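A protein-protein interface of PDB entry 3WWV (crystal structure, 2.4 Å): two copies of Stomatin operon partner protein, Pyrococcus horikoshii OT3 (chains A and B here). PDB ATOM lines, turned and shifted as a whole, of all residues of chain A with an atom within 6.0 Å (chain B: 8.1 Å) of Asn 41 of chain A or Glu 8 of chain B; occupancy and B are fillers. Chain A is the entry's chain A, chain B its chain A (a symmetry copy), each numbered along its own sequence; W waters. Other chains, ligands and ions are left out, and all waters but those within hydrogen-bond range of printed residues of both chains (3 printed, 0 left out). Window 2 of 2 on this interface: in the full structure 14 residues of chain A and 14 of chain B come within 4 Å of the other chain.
The side-chain hydroxyl (OG) of Ser 38 of chain A sits at hydrogen-bond distance from the backbone carbonyl oxygen (O) of Asn 41 of chain A (2.6 Å). The side-chain carboxylate (OE1) of Glu 9 of chain B lies within hydrogen-bond range of the backbone NH (N) of Gly 6 of chain B.
No position is printed for both chains. Of the 11 pairs that touch across the chains among the printed residues, none has its exchanged pair printed and touching as well.
NH2 of Arg 66 of chain A sits at hydrogen-bond distance from O of Glu 8 of chain B. The guanidinium group (NH2) of Arg 66 of chain A lies within hydrogen-bond range of the backbone carbonyl oxygen (O) of Glu 9 of chain B (2.8 Å). The guanidinium group (NH2) of Arg 66 of chain A is in hydrogen-bond range of the backbone carbonyl oxygen (O) of Ile 11 of chain B (2.8 Å).
Of the 11 printed residues of chain A, 4 touch a printed residue of chain B. Hydrophobic or aromatic side chains of chain A within 4 Å of the printed part of chain B: Phe 40. Hydrophobic or aromatic side chains of chain B that line the printed part of chain A: Ile 11 and Leu 13. Along chain B the printed residues that touch a printed residue of chain A span positions 7 to 13. Among the printed residues, no Asp or Glu carboxylate lies within 4 Å of a Lys or Arg side-chain nitrogen of the other chain.
Of chain A, only Phe 40 (3.6 Å), Asn 41 (3.9 Å) and Arg 66 (2.6 Å) come within 4 Å of Glu 8 of chain B. No residue of chain B comes within 4 Å of Gly 42 of chain A. Printed residues of chain A within 4 Å of Glu 9 of chain B: Arg 66 (2.8 Å). Printed residues of chain B within 4 Å of Lys 39 of chain A: Ile 11 (3.7 Å). Of the printed residues of chain A, Lys 7 of chain B touches Phe 40. Of the printed residues of chain A, Ile 11 of chain B touches Lys 39 (3.7 Å), Phe 40 (3.6 Å) and Arg 66 (2.8 Å). Of the printed residues of chain A, Gly 12 of chain B touches Arg 66. Met 55 of chain B touches none of the printed residues of chain A. Lys 43 of chain A touches none of the printed residues of chain B.
Ile 11 of chain B touches Lys 39 of chain A. Lys 7 of chain B touches Phe 40 of chain A. Phe 40 of chain A touches Glu 8 of chain B (CZ to CA, 3.6 Å). Ile 11 of chain B touches Phe 40 of chain A (CD1 to CZ, 3.6 Å). OE1 of Glu 8 of chain B touches ND2 of Asn 41 of chain A (3.9 Å). Arg 66 of chain A touches Met 10 of chain B (NH2 to N, 3.7 Å). Gly 12 of chain B touches Arg 66 of chain A. Leu 13 of chain B touches Arg 66 of chain A (CD2 to NH1, 3.8 Å).
Water W1 bridges NZ of Lys 39 of chain A (2.4 Å) and NZ of Lys 7 of chain B (2.6 Å). Water W2 lies within hydrogen-bond range of O of Glu 8 of chain B, O of Ile 11 of chain B and NH2 of Arg 66 of chain A. Water W3 bridges O of Gly 12 of chain B (3.0 Å) and N of Arg 66 of chain A (3.0 Å).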
ATOM      1  N   LEU A  21      -7.612  21.964  23.830  1.00  0.00           N
ATOM      2  CA  LEU A  21      -6.538  22.924  23.582  1.00  0.00           C
ATOM      3  C   LEU A  21      -6.943  23.860  22.456  1.00  0.00           C
ATOM      4  O   LEU A  21      -6.966  23.462  21.294  1.00  0.00           O
ATOM      5  CB  LEU A  21      -5.249  22.186  23.209  1.00  0.00           C
ATOM      6  CG  LEU A  21      -4.351  21.650  24.317  1.00  0.00           C
ATOM      7  CD1 LEU A  21      -5.109  20.927  25.421  1.00  0.00           C
ATOM      8  CD2 LEU A  21      -3.310  20.744  23.708  1.00  0.00           C
ATOM      9  N   PRO A  23      -5.905  27.648  21.774  1.00  0.00           N
ATOM     10  CA  PRO A  23      -4.804  26.677  21.736  1.00  0.00           C
ATOM     11  C   PRO A  23      -4.384  26.205  23.135  1.00  0.00           C
ATOM     12  O   PRO A  23      -3.630  25.236  23.250  1.00  0.00           O
ATOM     13  CB  PRO A  23      -3.672  27.473  21.077  1.00  0.00           C
ATOM     14  CG  PRO A  23      -3.909  28.878  21.510  1.00  0.00           C
ATOM     15  CD  PRO A  23      -5.390  29.036  21.765  1.00  0.00           C
ATOM     16  N   SER A  38      -1.049  23.977  22.466  1.00  0.00           N
ATOM     17  CA  SER A  38      -0.609  23.368  21.216  1.00  0.00           C
ATOM     18  C   SER A  38       0.359  24.303  20.513  1.00  0.00           C
ATOM     19  O   SER A  38       0.130  25.510  20.475  1.00  0.00           O
ATOM     20  CB  SER A  38      -1.781  23.034  20.306  1.00  0.00           C
ATOM     21  OG  SER A  38      -2.489  24.201  19.960  1.00  0.00           O
ATOM     22  N   LYS A  39       1.441  23.745  19.973  1.00  0.00           N
ATOM     23  CA  LYS A  39       2.487  24.564  19.357  1.00  0.00           C
ATOM     24  C   LYS A  39       2.049  25.300  18.089  1.00  0.00           C
ATOM     25  O   LYS A  39       2.369  26.472  17.929  1.00  0.00           O
ATOM     26  CB  LYS A  39       3.744  23.754  19.074  1.00  0.00           C
ATOM     27  CG  LYS A  39       4.944  24.646  18.771  1.00  0.00           C
ATOM     28  CD  LYS A  39       6.211  23.852  18.558  1.00  0.00           C
ATOM     29  CE  LYS A  39       7.278  24.746  17.959  1.00  0.00           C
ATOM     30  NZ  LYS A  39       7.915  25.623  18.975  1.00  0.00           N
ATOM     31  N   PHE A  40       1.328  24.625  17.196  1.00  0.00           N
ATOM     32  CA  PHE A  40       0.939  25.249  15.924  1.00  0.00           C
ATOM     33  C   PHE A  40      -0.561  25.314  15.767  1.00  0.00           C
ATOM     34  O   PHE A  40      -1.102  26.367  15.412  1.00  0.00           O
ATOM     35  CB  PHE A  40       1.454  24.465  14.718  1.00  0.00           C
ATOM     36  CG  PHE A  40       2.879  24.063  14.812  1.00  0.00           C
ATOM     37  CD1 PHE A  40       3.886  24.958  14.480  1.00  0.00           C
ATOM     38  CD2 PHE A  40       3.214  22.769  15.192  1.00  0.00           C
ATOM     39  CE1 PHE A  40       5.211  24.575  14.547  1.00  0.00           C
ATOM     40  CE2 PHE A  40       4.534  22.378  15.254  1.00  0.00           C
ATOM     41  CZ  PHE A  40       5.531  23.283  14.939  1.00  0.00           C
ATOM     42  N   ASN A  41      -1.201  24.157  15.991  1.00  0.00           N
ATOM     43  CA  ASN A  41      -2.637  23.959  15.787  1.00  0.00           C
ATOM     44  C   ASN A  41      -3.480  24.960  16.552  1.00  0.00           C
ATOM     45  O   ASN A  41      -3.164  25.309  17.683  1.00  0.00           O
ATOM     46  CB  ASN A  41      -3.056  22.537  16.184  1.00  0.00           C
ATOM     47  CG  ASN A  41      -2.731  21.493  15.120  1.00  0.00           C
ATOM     48  OD1 ASN A  41      -2.973  20.298  15.321  1.00  0.00           O
ATOM     49  ND2 ASN A  41      -2.187  21.934  13.982  1.00  0.00           N
ATOM     50  N   GLY A  42      -4.553  25.421  15.924  1.00  0.00           N
ATOM     51  CA  GLY A  42      -5.493  26.317  16.581  1.00  0.00           C
ATOM     52  C   GLY A  42      -6.337  25.603  17.628  1.00  0.00           C
ATOM     53  O   GLY A  42      -6.822  26.252  18.565  1.00  0.00           O
ATOM     54  N   LYS A  43      -6.497  24.278  17.476  1.00  0.00           N
ATOM     55  CA  LYS A  43      -7.427  23.488  18.299  1.00  0.00           C
ATOM     56  C   LYS A  43      -7.139  21.976  18.301  1.00  0.00           C
ATOM     57  O   LYS A  43      -7.182  21.327  17.253  1.00  0.00           O
ATOM     58  CB  LYS A  43      -8.876  23.737  17.852  1.00  0.00           C
ATOM     59  CG  LYS A  43      -9.928  22.944  18.619  1.00  0.00           C
ATOM     60  CD  LYS A  43     -11.267  22.953  17.898  1.00  0.00           C
ATOM     61  CE  LYS A  43     -11.995  24.265  18.126  1.00  0.00           C
ATOM     62  NZ  LYS A  43     -13.070  24.481  17.121  1.00  0.00           N
ATOM     63  N   ILE A  44      -6.857  21.428  19.482  1.00  0.00           N
ATOM     64  CA  ILE A  44      -6.743  19.980  19.671  1.00  0.00           C
ATOM     65  C   ILE A  44      -7.820  19.500  20.656  1.00  0.00           C
ATOM     66  O   ILE A  44      -7.914  19.992  21.773  1.00  0.00           O
ATOM     67  CB  ILE A  44      -5.326  19.557  20.129  1.00  0.00           C
ATOM     68  CG1 ILE A  44      -4.263  20.093  19.155  1.00  0.00           C
ATOM     69  CG2 ILE A  44      -5.233  18.040  20.252  1.00  0.00           C
ATOM     70  CD1 ILE A  44      -2.836  19.764  19.551  1.00  0.00           C
ATOM     71  N   ARG A  64      -0.221  17.359  18.318  1.00  0.00           N
ATOM     72  CA  ARG A  64      -0.960  16.096  18.311  1.00  0.00           C
ATOM     73  C   ARG A  64      -0.065  14.978  17.832  1.00  0.00           C
ATOM     74  O   ARG A  64       0.804  15.180  16.985  1.00  0.00           O
ATOM     75  CB  ARG A  64      -2.281  16.116  17.528  1.00  0.00           C
ATOM     76  CG  ARG A  64      -2.360  17.009  16.309  1.00  0.00           C
ATOM     77  CD  ARG A  64      -3.530  16.592  15.415  1.00  0.00           C
ATOM     78  NE  ARG A  64      -4.724  16.200  16.152  1.00  0.00           N
ATOM     79  CZ  ARG A  64      -5.762  16.998  16.388  1.00  0.00           C
ATOM     80  NH1 ARG A  64      -5.779  18.243  15.948  1.00  0.00           N
ATOM     81  NH2 ARG A  64      -6.791  16.542  17.076  1.00  0.00           N
ATOM     82  N   ARG A  66       1.532  12.034  15.939  1.00  0.00           N
ATOM     83  CA  ARG A  66       1.537  11.669  14.519  1.00  0.00           C
ATOM     84  C   ARG A  66       0.923  10.294  14.243  1.00  0.00           C
ATOM     85  O   ARG A  66       1.080   9.357  15.034  1.00  0.00           O
ATOM     86  CB  ARG A  66       2.953  11.729  13.956  1.00  0.00           C
ATOM     87  CG  ARG A  66       3.590  13.107  14.036  1.00  0.00           C
ATOM     88  CD  ARG A  66       3.237  13.962  12.833  1.00  0.00           C
ATOM     89  NE  ARG A  66       3.956  15.226  12.895  1.00  0.00           N
ATOM     90  CZ  ARG A  66       4.405  15.907  11.845  1.00  0.00           C
ATOM     91  NH1 ARG A  66       4.224  15.460  10.607  1.00  0.00           N
ATOM     92  NH2 ARG A  66       5.040  17.051  12.044  1.00  0.00           N
ATOM     93  N   THR B   5      11.324  23.806   4.537  1.00  0.00           N
ATOM     94  CA  THR B   5      10.503  22.744   5.156  1.00  0.00           C
ATOM     95  C   THR B   5      10.254  23.098   6.627  1.00  0.00           C
ATOM     96  O   THR B   5      11.145  22.952   7.463  1.00  0.00           O
ATOM     97  CB  THR B   5      11.169  21.344   5.065  1.00  0.00           C
ATOM     98  OG1 THR B   5      11.319  20.965   3.692  1.00  0.00           O
ATOM     99  CG2 THR B   5      10.329  20.284   5.773  1.00  0.00           C
ATOM    100  N   GLY B   6       9.041  23.562   6.927  1.00  0.00           N
ATOM    101  CA  GLY B   6       8.723  24.168   8.223  1.00  0.00           C
ATOM    102  C   GLY B   6       8.837  23.272   9.440  1.00  0.00           C
ATOM    103  O   GLY B   6       8.988  22.058   9.329  1.00  0.00           O
ATOM    104  N   LYS B   7       8.759  23.894  10.614  1.00  0.00           N
ATOM    105  CA  LYS B   7       8.760  23.188  11.896  1.00  0.00           C
ATOM    106  C   LYS B   7       7.571  22.241  12.037  1.00  0.00           C
ATOM    107  O   LYS B   7       7.683  21.160  12.621  1.00  0.00           O
ATOM    108  CB  LYS B   7       8.756  24.188  13.050  1.00  0.00           C
ATOM    109  CG  LYS B   7      10.052  24.953  13.229  1.00  0.00           C
ATOM    110  CD  LYS B   7      10.059  25.653  14.573  1.00  0.00           C
ATOM    111  CE  LYS B   7      11.287  26.532  14.729  1.00  0.00           C
ATOM    112  NZ  LYS B   7      11.308  27.187  16.066  1.00  0.00           N
ATOM    113  N   GLU B   8       6.436  22.657  11.490  1.00  0.00           N
ATOM    114  CA  GLU B   8       5.197  21.920  11.626  1.00  0.00           C
ATOM    115  C   GLU B   8       5.288  20.531  10.996  1.00  0.00           C
ATOM    116  O   GLU B   8       4.672  19.587  11.477  1.00  0.00           O
ATOM    117  CB  GLU B   8       4.052  22.722  11.015  1.00  0.00           C
ATOM    118  CG  GLU B   8       2.679  22.225  11.427  1.00  0.00           C
ATOM    119  CD  GLU B   8       1.578  23.241  11.180  1.00  0.00           C
ATOM    120  OE1 GLU B   8       0.395  22.844  11.258  1.00  0.00           O
ATOM    121  OE2 GLU B   8       1.887  24.428  10.917  1.00  0.00           O
ATOM    122  N   GLU B   9       6.066  20.417   9.928  1.00  0.00           N
ATOM    123  CA  GLU B   9       6.189  19.167   9.193  1.00  0.00           C
ATOM    124  C   GLU B   9       7.054  18.169   9.949  1.00  0.00           C
ATOM    125  O   GLU B   9       6.812  16.967   9.882  1.00  0.00           O
ATOM    126  CB  GLU B   9       6.784  19.411   7.802  1.00  0.00           C
ATOM    127  CG  GLU B   9       6.172  20.580   7.044  1.00  0.00           C
ATOM    128  CD  GLU B   9       6.815  20.795   5.682  1.00  0.00           C
ATOM    129  OE1 GLU B   9       7.280  21.927   5.418  1.00  0.00           O
ATOM    130  OE2 GLU B   9       6.870  19.834   4.878  1.00  0.00           O
ATOM    131  N   MET B  10       8.055  18.665  10.668  1.00  0.00           N
ATOM    132  CA  MET B  10       9.072  17.794  11.273  1.00  0.00           C
ATOM    133  C   MET B  10       8.814  17.446  12.738  1.00  0.00           C
ATOM    134  O   MET B  10       9.153  16.347  13.180  1.00  0.00           O
ATOM    135  CB  MET B  10      10.477  18.406  11.147  1.00  0.00           C
ATOM    136  CG  MET B  10      10.930  18.722   9.727  1.00  0.00           C
ATOM    137  SD  MET B  10      10.756  17.312   8.634  1.00  0.00           S
ATOM    138  CE  MET B  10      11.980  16.172   9.285  1.00  0.00           C
ATOM    139  N   ILE B  11       8.225  18.378  13.481  1.00  0.00           N
ATOM    140  CA  ILE B  11       8.073  18.218  14.914  1.00  0.00           C
ATOM    141  C   ILE B  11       7.092  17.085  15.250  1.00  0.00           C
ATOM    142  O   ILE B  11       5.993  17.001  14.698  1.00  0.00           O
ATOM    143  CB  ILE B  11       7.736  19.570  15.600  1.00  0.00           C
ATOM    144  CG1 ILE B  11       8.954  20.495  15.513  1.00  0.00           C
ATOM    145  CG2 ILE B  11       7.359  19.366  17.062  1.00  0.00           C
ATOM    146  CD1 ILE B  11       8.725  21.901  16.022  1.00  0.00           C
ATOM    147  N   GLY B  12       7.519  16.187  16.132  1.00  0.00           N
ATOM    148  CA  GLY B  12       6.697  15.040  16.508  1.00  0.00           C
ATOM    149  C   GLY B  12       7.066  13.748  15.814  1.00  0.00           C
ATOM    150  O   GLY B  12       6.689  12.678  16.278  1.00  0.00           O
ATOM    151  N   LEU B  13       7.790  13.836  14.697  1.00  0.00           N
ATOM    152  CA  LEU B  13       8.197  12.634  13.950  1.00  0.00           C
ATOM    153  C   LEU B  13       9.255  11.819  14.689  1.00  0.00           C
ATOM    154  O   LEU B  13      10.005  12.352  15.516  1.00  0.00           O
ATOM    155  CB  LEU B  13       8.727  12.995  12.553  1.00  0.00           C
ATOM    156  CG  LEU B  13       7.728  13.548  11.529  1.00  0.00           C
ATOM    157  CD1 LEU B  13       8.418  13.909  10.223  1.00  0.00           C
ATOM    158  CD2 LEU B  13       6.578  12.579  11.281  1.00  0.00           C
ATOM    159  N   MET B  55      13.097  22.661  15.969  1.00  0.00           N
ATOM    160  CA  MET B  55      13.983  22.850  14.829  1.00  0.00           C
ATOM    161  C   MET B  55      14.743  24.162  14.953  1.00  0.00           C
ATOM    162  O   MET B  55      14.181  25.181  15.337  1.00  0.00           O
ATOM    163  CB  MET B  55      13.193  22.834  13.528  1.00  0.00           C
ATOM    164  CG  MET B  55      13.887  22.076  12.418  1.00  0.00           C
ATOM    165  SD  MET B  55      13.027  22.197  10.846  1.00  0.00           S
ATOM    166  CE  MET B  55      11.407  21.674  11.343  1.00  0.00           C
HETATM  167  O   HOH W   1       9.986  26.685  18.222  1.00  0.00           O
HETATM  168  O   HOH W   2       3.993  18.934  14.106  1.00  0.00           O
HETATM  169  O   HOH W   3       4.003  12.642  17.545  1.00  0.00           O
